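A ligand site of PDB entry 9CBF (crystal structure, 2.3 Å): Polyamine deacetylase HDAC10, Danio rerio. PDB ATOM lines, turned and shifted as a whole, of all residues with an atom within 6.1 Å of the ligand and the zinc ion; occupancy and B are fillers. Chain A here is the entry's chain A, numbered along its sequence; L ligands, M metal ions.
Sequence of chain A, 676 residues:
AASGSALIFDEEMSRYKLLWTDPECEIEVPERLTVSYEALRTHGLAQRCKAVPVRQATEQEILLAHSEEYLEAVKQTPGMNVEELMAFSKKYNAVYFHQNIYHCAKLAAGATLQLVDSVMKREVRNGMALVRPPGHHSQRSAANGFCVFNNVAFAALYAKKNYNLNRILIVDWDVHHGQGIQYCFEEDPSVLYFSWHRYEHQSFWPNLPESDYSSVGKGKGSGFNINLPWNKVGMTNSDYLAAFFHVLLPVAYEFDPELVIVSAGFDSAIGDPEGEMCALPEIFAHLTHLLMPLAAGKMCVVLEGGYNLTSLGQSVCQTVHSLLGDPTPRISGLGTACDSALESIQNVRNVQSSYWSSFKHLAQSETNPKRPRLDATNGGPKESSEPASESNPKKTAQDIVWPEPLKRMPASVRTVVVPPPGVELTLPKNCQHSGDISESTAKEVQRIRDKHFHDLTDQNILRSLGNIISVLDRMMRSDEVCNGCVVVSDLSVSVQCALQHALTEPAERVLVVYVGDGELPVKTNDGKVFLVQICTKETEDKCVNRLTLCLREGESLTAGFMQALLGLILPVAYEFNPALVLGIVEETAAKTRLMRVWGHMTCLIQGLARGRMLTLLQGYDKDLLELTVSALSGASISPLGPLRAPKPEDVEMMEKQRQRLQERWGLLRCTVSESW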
ATOM      1  N   GLU A  24       7.769   8.057 -17.413  1.00  0.00           N
ATOM      2  CA  GLU A  24       8.538   7.427 -16.354  1.00  0.00           C
ATOM      3  C   GLU A  24       9.683   8.312 -15.881  1.00  0.00           C
ATOM      4  O   GLU A  24      10.023   8.304 -14.694  1.00  0.00           O
ATOM      5  CB  GLU A  24       9.066   6.068 -16.829  1.00  0.00           C
ATOM      6  CG  GLU A  24       9.601   5.180 -15.730  1.00  0.00           C
ATOM      7  CD  GLU A  24       9.825   3.753 -16.188  1.00  0.00           C
ATOM      8  OE1 GLU A  24      10.054   3.545 -17.398  1.00  0.00           O
ATOM      9  OE2 GLU A  24       9.769   2.833 -15.341  1.00  0.00           O
ATOM     10  N   CYS A  25      10.284   9.083 -16.785  1.00  0.00           N
ATOM     11  CA  CYS A  25      11.439   9.904 -16.472  1.00  0.00           C
ATOM     12  C   CYS A  25      11.108  11.385 -16.343  1.00  0.00           C
ATOM     13  O   CYS A  25      12.019  12.190 -16.098  1.00  0.00           O
ATOM     14  CB  CYS A  25      12.525   9.715 -17.540  1.00  0.00           C
ATOM     15  SG  CYS A  25      13.130   8.025 -17.714  1.00  0.00           S
ATOM     16  N   ILE A  27       9.911  13.055 -14.051  1.00  0.00           N
ATOM     17  CA  ILE A  27      10.135  13.628 -12.731  1.00  0.00           C
ATOM     18  C   ILE A  27      11.571  14.118 -12.574  1.00  0.00           C
ATOM     19  O   ILE A  27      11.821  15.077 -11.840  1.00  0.00           O
ATOM     20  CB  ILE A  27       9.785  12.603 -11.644  1.00  0.00           C
ATOM     21  CG1 ILE A  27      10.549  11.295 -11.899  1.00  0.00           C
ATOM     22  CG2 ILE A  27       8.294  12.353 -11.607  1.00  0.00           C
ATOM     23  CD1 ILE A  27      10.469  10.311 -10.774  1.00  0.00           C
ATOM     24  N   ASN A  93      16.731   0.606 -18.940  1.00  0.00           N
ATOM     25  CA  ASN A  93      15.456   0.694 -18.242  1.00  0.00           C
ATOM     26  C   ASN A  93      15.395   1.957 -17.398  1.00  0.00           C
ATOM     27  O   ASN A  93      16.281   2.196 -16.576  1.00  0.00           O
ATOM     28  CB  ASN A  93      15.229  -0.535 -17.360  1.00  0.00           C
ATOM     29  CG  ASN A  93      13.993  -0.406 -16.496  1.00  0.00           C
ATOM     30  OD1 ASN A  93      14.067  -0.501 -15.267  1.00  0.00           O
ATOM     31  ND2 ASN A  93      12.846  -0.184 -17.117  1.00  0.00           N
ATOM     32  N   ALA A  94      14.355   2.764 -17.618  1.00  0.00           N
ATOM     33  CA  ALA A  94      14.044   3.924 -16.786  1.00  0.00           C
ATOM     34  C   ALA A  94      15.193   4.933 -16.757  1.00  0.00           C
ATOM     35  O   ALA A  94      15.607   5.413 -15.701  1.00  0.00           O
ATOM     36  CB  ALA A  94      13.658   3.496 -15.368  1.00  0.00           C
ATOM     37  N   PRO A 134      21.786  11.116 -10.541  1.00  0.00           N
ATOM     38  CA  PRO A 134      22.052  10.234  -9.399  1.00  0.00           C
ATOM     39  C   PRO A 134      22.823   8.989  -9.827  1.00  0.00           C
ATOM     40  O   PRO A 134      23.140   8.843 -11.011  1.00  0.00           O
ATOM     41  CB  PRO A 134      20.652   9.883  -8.883  1.00  0.00           C
ATOM     42  CG  PRO A 134      19.752  10.115 -10.045  1.00  0.00           C
ATOM     43  CD  PRO A 134      20.336  11.263 -10.800  1.00  0.00           C
ATOM     44  N   HIS A 136      22.891   5.535  -7.623  1.00  0.00           N
ATOM     45  CA  HIS A 136      22.790   4.277  -6.890  1.00  0.00           C
ATOM     46  C   HIS A 136      22.118   3.144  -7.678  1.00  0.00           C
ATOM     47  O   HIS A 136      22.216   1.998  -7.263  1.00  0.00           O
ATOM     48  CB  HIS A 136      22.062   4.491  -5.561  1.00  0.00           C
ATOM     49  CG  HIS A 136      20.606   4.829  -5.686  1.00  0.00           C
ATOM     50  ND1 HIS A 136      19.688   4.478  -4.729  1.00  0.00           N
ATOM     51  CD2 HIS A 136      19.924   5.500  -6.646  1.00  0.00           C
ATOM     52  CE1 HIS A 136      18.483   4.906  -5.090  1.00  0.00           C
ATOM     53  NE2 HIS A 136      18.606   5.522  -6.255  1.00  0.00           N
ATOM     54  N   HIS A 137      21.463   3.444  -8.800  1.00  0.00           N
ATOM     55  CA  HIS A 137      20.881   2.373  -9.613  1.00  0.00           C
ATOM     56  C   HIS A 137      21.801   1.898 -10.733  1.00  0.00           C
ATOM     57  O   HIS A 137      21.689   0.749 -11.153  1.00  0.00           O
ATOM     58  CB  HIS A 137      19.548   2.824 -10.230  1.00  0.00           C
ATOM     59  CG  HIS A 137      18.469   3.071  -9.224  1.00  0.00           C
ATOM     60  ND1 HIS A 137      18.029   2.091  -8.353  1.00  0.00           N
ATOM     61  CD2 HIS A 137      17.730   4.166  -8.960  1.00  0.00           C
ATOM     62  CE1 HIS A 137      17.074   2.582  -7.587  1.00  0.00           C
ATOM     63  NE2 HIS A 137      16.870   3.839  -7.942  1.00  0.00           N
ATOM     64  N   ASN A 144      20.662   2.804 -15.411  1.00  0.00           N
ATOM     65  CA  ASN A 144      19.432   2.310 -14.836  1.00  0.00           C
ATOM     66  C   ASN A 144      18.878   3.340 -13.861  1.00  0.00           C
ATOM     67  O   ASN A 144      19.642   3.988 -13.145  1.00  0.00           O
ATOM     68  CB  ASN A 144      19.667   0.978 -14.115  1.00  0.00           C
ATOM     69  CG  ASN A 144      18.378   0.260 -13.774  1.00  0.00           C
ATOM     70  OD1 ASN A 144      17.906   0.336 -12.648  1.00  0.00           O
ATOM     71  ND2 ASN A 144      17.820  -0.456 -14.742  1.00  0.00           N
ATOM     72  N   GLY A 145      17.556   3.491 -13.857  1.00  0.00           N
ATOM     73  CA  GLY A 145      16.865   4.349 -12.916  1.00  0.00           C
ATOM     74  C   GLY A 145      17.406   5.763 -12.797  1.00  0.00           C
ATOM     75  O   GLY A 145      17.791   6.188 -11.706  1.00  0.00           O
ATOM     76  N   PHE A 146      17.433   6.486 -13.920  1.00  0.00           N
ATOM     77  CA  PHE A 146      17.915   7.862 -14.046  1.00  0.00           C
ATOM     78  C   PHE A 146      19.422   7.988 -13.847  1.00  0.00           C
ATOM     79  O   PHE A 146      19.949   9.102 -13.877  1.00  0.00           O
ATOM     80  CB  PHE A 146      17.245   8.833 -13.060  1.00  0.00           C
ATOM     81  CG  PHE A 146      15.741   8.801 -13.095  1.00  0.00           C
ATOM     82  CD1 PHE A 146      15.055   8.377 -14.210  1.00  0.00           C
ATOM     83  CD2 PHE A 146      15.028   9.223 -11.992  1.00  0.00           C
ATOM     84  CE1 PHE A 146      13.674   8.354 -14.218  1.00  0.00           C
ATOM     85  CE2 PHE A 146      13.641   9.205 -11.995  1.00  0.00           C
ATOM     86  CZ  PHE A 146      12.964   8.770 -13.108  1.00  0.00           C
ATOM     87  N   CYS A 147      20.132   6.877 -13.635  1.00  0.00           N
ATOM     88  CA  CYS A 147      21.540   6.919 -13.260  1.00  0.00           C
ATOM     89  C   CYS A 147      22.418   6.457 -14.420  1.00  0.00           C
ATOM     90  O   CYS A 147      22.102   5.480 -15.107  1.00  0.00           O
ATOM     91  CB  CYS A 147      21.798   6.048 -12.031  1.00  0.00           C
ATOM     92  SG  CYS A 147      20.738   6.430 -10.615  1.00  0.00           S
ATOM     93  N   ASP A 174      17.287   6.763  -0.035  1.00  0.00           N
ATOM     94  CA  ASP A 174      16.402   6.985  -1.171  1.00  0.00           C
ATOM     95  C   ASP A 174      15.280   5.956  -1.134  1.00  0.00           C
ATOM     96  O   ASP A 174      15.472   4.814  -0.722  1.00  0.00           O
ATOM     97  CB  ASP A 174      17.198   6.884  -2.471  1.00  0.00           C
ATOM     98  CG  ASP A 174      16.378   7.257  -3.689  1.00  0.00           C
ATOM     99  OD1 ASP A 174      15.468   6.492  -4.058  1.00  0.00           O
ATOM    100  OD2 ASP A 174      16.646   8.320  -4.283  1.00  0.00           O
ATOM    101  N   VAL A 175      14.079   6.378  -1.539  1.00  0.00           N
ATOM    102  CA  VAL A 175      12.928   5.492  -1.471  1.00  0.00           C
ATOM    103  C   VAL A 175      13.030   4.314  -2.434  1.00  0.00           C
ATOM    104  O   VAL A 175      12.265   3.349  -2.298  1.00  0.00           O
ATOM    105  CB  VAL A 175      11.615   6.263  -1.738  1.00  0.00           C
ATOM    106  CG1 VAL A 175      11.366   6.394  -3.236  1.00  0.00           C
ATOM    107  CG2 VAL A 175      10.443   5.579  -1.049  1.00  0.00           C
ATOM    108  N   HIS A 176      13.959   4.365  -3.387  1.00  0.00           N
ATOM    109  CA  HIS A 176      14.235   3.241  -4.258  1.00  0.00           C
ATOM    110  C   HIS A 176      15.447   2.473  -3.754  1.00  0.00           C
ATOM    111  O   HIS A 176      16.289   2.997  -3.012  1.00  0.00           O
ATOM    112  CB  HIS A 176      14.471   3.717  -5.695  1.00  0.00           C
ATOM    113  CG  HIS A 176      13.320   4.462  -6.285  1.00  0.00           C
ATOM    114  ND1 HIS A 176      13.090   5.792  -6.028  1.00  0.00           N
ATOM    115  CD2 HIS A 176      12.319   4.059  -7.105  1.00  0.00           C
ATOM    116  CE1 HIS A 176      12.004   6.184  -6.681  1.00  0.00           C
ATOM    117  NE2 HIS A 176      11.518   5.154  -7.334  1.00  0.00           N
ATOM    118  N   PHE A 204       6.915  -2.812  -6.665  1.00  0.00           N
ATOM    119  CA  PHE A 204       7.412  -1.484  -6.979  1.00  0.00           C
ATOM    120  C   PHE A 204       8.785  -1.573  -7.635  1.00  0.00           C
ATOM    121  O   PHE A 204       9.562  -2.513  -7.380  1.00  0.00           O
ATOM    122  CB  PHE A 204       7.473  -0.604  -5.734  1.00  0.00           C
ATOM    123  CG  PHE A 204       7.695   0.852  -6.032  1.00  0.00           C
ATOM    124  CD1 PHE A 204       6.686   1.618  -6.605  1.00  0.00           C
ATOM    125  CD2 PHE A 204       8.900   1.463  -5.753  1.00  0.00           C
ATOM    126  CE1 PHE A 204       6.881   2.949  -6.892  1.00  0.00           C
ATOM    127  CE2 PHE A 204       9.112   2.802  -6.028  1.00  0.00           C
ATOM    128  CZ  PHE A 204       8.091   3.549  -6.597  1.00  0.00           C
ATOM    129  N   TRP A 205       9.087  -0.590  -8.472  1.00  0.00           N
ATOM    130  CA  TRP A 205      10.339  -0.577  -9.219  1.00  0.00           C
ATOM    131  C   TRP A 205      11.516  -0.566  -8.247  1.00  0.00           C
ATOM    132  O   TRP A 205      11.490   0.151  -7.235  1.00  0.00           O
ATOM    133  CB  TRP A 205      10.381   0.637 -10.137  1.00  0.00           C
ATOM    134  CG  TRP A 205      11.480   0.613 -11.147  1.00  0.00           C
ATOM    135  CD1 TRP A 205      11.390   0.172 -12.435  1.00  0.00           C
ATOM    136  CD2 TRP A 205      12.831   1.030 -10.948  1.00  0.00           C
ATOM    137  NE1 TRP A 205      12.619   0.288 -13.054  1.00  0.00           N
ATOM    138  CE2 TRP A 205      13.517   0.808 -12.157  1.00  0.00           C
ATOM    139  CE3 TRP A 205      13.536   1.549  -9.863  1.00  0.00           C
ATOM    140  CZ2 TRP A 205      14.862   1.105 -12.315  1.00  0.00           C
ATOM    141  CZ3 TRP A 205      14.867   1.844 -10.017  1.00  0.00           C
ATOM    142  CH2 TRP A 205      15.527   1.624 -11.240  1.00  0.00           C
ATOM    143  N   GLY A 265      18.726  10.254  -1.146  1.00  0.00           N
ATOM    144  CA  GLY A 265      17.585  10.468  -2.001  1.00  0.00           C
ATOM    145  C   GLY A 265      16.404  10.888  -1.145  1.00  0.00           C
ATOM    146  O   GLY A 265      16.006  10.181  -0.227  1.00  0.00           O
ATOM    147  N   ASP A 267      13.313  11.410  -2.195  1.00  0.00           N
ATOM    148  CA  ASP A 267      12.016  10.921  -2.637  1.00  0.00           C
ATOM    149  C   ASP A 267      11.312  10.100  -1.556  1.00  0.00           C
ATOM    150  O   ASP A 267      10.143   9.750  -1.732  1.00  0.00           O
ATOM    151  CB  ASP A 267      12.170  10.088  -3.909  1.00  0.00           C
ATOM    152  CG  ASP A 267      13.339   9.130  -3.847  1.00  0.00           C
ATOM    153  OD1 ASP A 267      14.025   9.094  -2.807  1.00  0.00           O
ATOM    154  OD2 ASP A 267      13.555   8.412  -4.836  1.00  0.00           O
ATOM    155  N   GLU A 274       6.882   9.765  -6.097  1.00  0.00           N
ATOM    156  CA  GLU A 274       7.388   8.389  -6.300  1.00  0.00           C
ATOM    157  C   GLU A 274       7.394   7.614  -4.985  1.00  0.00           C
ATOM    158  O   GLU A 274       7.013   6.440  -4.981  1.00  0.00           O
ATOM    159  CB  GLU A 274       8.803   8.434  -6.854  1.00  0.00           C
ATOM    160  CG  GLU A 274       8.850   8.429  -8.367  1.00  0.00           C
ATOM    161  CD  GLU A 274       8.553   7.054  -8.917  1.00  0.00           C
ATOM    162  OE1 GLU A 274       9.250   6.095  -8.523  1.00  0.00           O
ATOM    163  OE2 GLU A 274       7.630   6.933  -9.747  1.00  0.00           O
ATOM    164  N   GLU A 304      20.784  11.775  -4.385  1.00  0.00           N
ATOM    165  CA  GLU A 304      20.276  10.757  -5.286  1.00  0.00           C
ATOM    166  C   GLU A 304      18.953  11.268  -5.840  1.00  0.00           C
ATOM    167  O   GLU A 304      18.944  12.112  -6.744  1.00  0.00           O
ATOM    168  CB  GLU A 304      20.157   9.404  -4.575  1.00  0.00           C
ATOM    169  CG  GLU A 304      21.481   8.857  -4.058  1.00  0.00           C
ATOM    170  CD  GLU A 304      22.238   8.069  -5.112  1.00  0.00           C
ATOM    171  OE1 GLU A 304      21.747   7.957  -6.255  1.00  0.00           O
ATOM    172  OE2 GLU A 304      23.333   7.548  -4.790  1.00  0.00           O
ATOM    173  N   GLY A 305      17.823  10.790  -5.326  1.00  0.00           N
ATOM    174  CA  GLY A 305      16.518  11.171  -5.811  1.00  0.00           C
ATOM    175  C   GLY A 305      15.897  12.302  -5.021  1.00  0.00           C
ATOM    176  O   GLY A 305      16.571  13.017  -4.256  1.00  0.00           O
ATOM    177  N   GLY A 306      14.590  12.459  -5.182  1.00  0.00           N
ATOM    178  CA  GLY A 306      13.862  13.582  -4.613  1.00  0.00           C
ATOM    179  C   GLY A 306      13.268  14.452  -5.692  1.00  0.00           C
ATOM    180  O   GLY A 306      13.989  15.186  -6.373  1.00  0.00           O
ATOM    181  N   TYR A 307      11.948  14.376  -5.882  1.00  0.00           N
ATOM    182  CA  TYR A 307      11.324  14.934  -7.064  1.00  0.00           C
ATOM    183  C   TYR A 307      10.164  15.879  -6.786  1.00  0.00           C
ATOM    184  O   TYR A 307       9.541  16.364  -7.742  1.00  0.00           O
ATOM    185  CB  TYR A 307      10.853  13.792  -7.987  1.00  0.00           C
ATOM    186  CG  TYR A 307      11.970  12.819  -8.269  1.00  0.00           C
ATOM    187  CD1 TYR A 307      12.891  13.066  -9.287  1.00  0.00           C
ATOM    188  CD2 TYR A 307      12.129  11.677  -7.507  1.00  0.00           C
ATOM    189  CE1 TYR A 307      13.925  12.189  -9.539  1.00  0.00           C
ATOM    190  CE2 TYR A 307      13.159  10.788  -7.753  1.00  0.00           C
ATOM    191  CZ  TYR A 307      14.050  11.049  -8.763  1.00  0.00           C
ATOM    192  OH  TYR A 307      15.077  10.166  -9.018  1.00  0.00           O
HETATM  193  C1  LIG L   1      10.007   5.849 -12.119  1.00  0.00           C
HETATM  194  C2  LIG L   1      11.411   5.612 -11.706  1.00  0.00           C
HETATM  195  C3  LIG L   1      12.142   4.588 -12.309  1.00  0.00           C
HETATM  196  C4  LIG L   1      13.479   4.343 -11.930  1.00  0.00           C
HETATM  197  C5  LIG L   1      14.086   5.147 -10.931  1.00  0.00           C
HETATM  198  C6  LIG L   1      13.376   6.138 -10.345  1.00  0.00           C
HETATM  199  C7  LIG L   1      14.077   7.005  -9.247  1.00  0.00           C
HETATM  200  C8  LIG L   1      15.467   6.708  -8.883  1.00  0.00           C
HETATM  201  C9  LIG L   1      11.997   6.390 -10.744  1.00  0.00           C
HETATM  202  N1  LIG L   1       9.113   5.244 -11.204  1.00  0.00           N
HETATM  203  O1  LIG L   1      13.494   7.893  -8.722  1.00  0.00           O
HETATM  204  S1  LIG L   1      16.089   7.864  -7.573  1.00  0.00           S
HETATM  205 ZN    ZN M   1      14.862   7.244  -5.767  1.00  0.00          ZN
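A nitrogen (N1) of the ligand lies within salt-bridge range of the side-chain carboxylate (OE2) of Glu 274, at 2.7 Å.
The side-chain hydroxyl (OH) of Tyr 307 lies within hydrogen-bond range of an oxygen (O1) of the ligand, 2.8 Å away.
S1 of the ligand sits close to NE2 of His 136.
O of Glu 24 touches C1 of the ligand, 3.6 Å away.
CB of Ala 94 touches C4 of the ligand, 3.5 Å away.
His 137 touches the ligand.
Gly 145 touches the ligand (CA to C5, 3.5 Å).
CZ of Phe 146 touches C9 of the ligand, 3.5 Å away.
Trp 205 touches the ligand (CZ3 to C4, 3.4 Å).
Gly 305 touches the ligand (CA to S1, 3.8 Å).
Hydrophobic or aromatic side chains within 4 Å of the ligand: Ala 94, His 137, Phe 146, His 176, Trp 205 and Tyr 307.
The nearest printed residue that does not touch the ligand is Ile 27 (4.2 Å).
Three residues have an atom within 4 Å of the zinc ion: Asp 174, His 176 and Asp 267.
The zinc ion is bound by OD1 of Asp 174, OD2 of Asp 267, S1 of the ligand, ND1 of His 176 and OD2 of Asp 174.
The zinc ion has five donor atoms within binding distance.
The backbone NH of Val 175 lies within hydrogen-bond range of the side-chain carboxylate of Asp 267 (3.0 Å).
The side-chain carboxylate (OE1) of Glu 274 sits at hydrogen-bond distance from a ring nitrogen (NE2) of His 176, 2.7 Å away.
N of His 137 sits at hydrogen-bond distance from SG of Cys 147.
The backbone NH (N) of Phe 146 is in hydrogen-bond range of the backbone carbonyl oxygen (O) of Ala 94 (2.8 Å).
N of Gly 145 lies close to O of Ala 94.
O of Gly 145 sits at hydrogen-bond distance from SG of Cys 147 (3.2 Å).
O of Asn 93 lies within hydrogen-bond range of N of Gly 145.
The side-chain sulfur (SG) of Cys 147 sits at hydrogen-bond distance from the backbone NH (N) of His 136 (3.8 Å).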
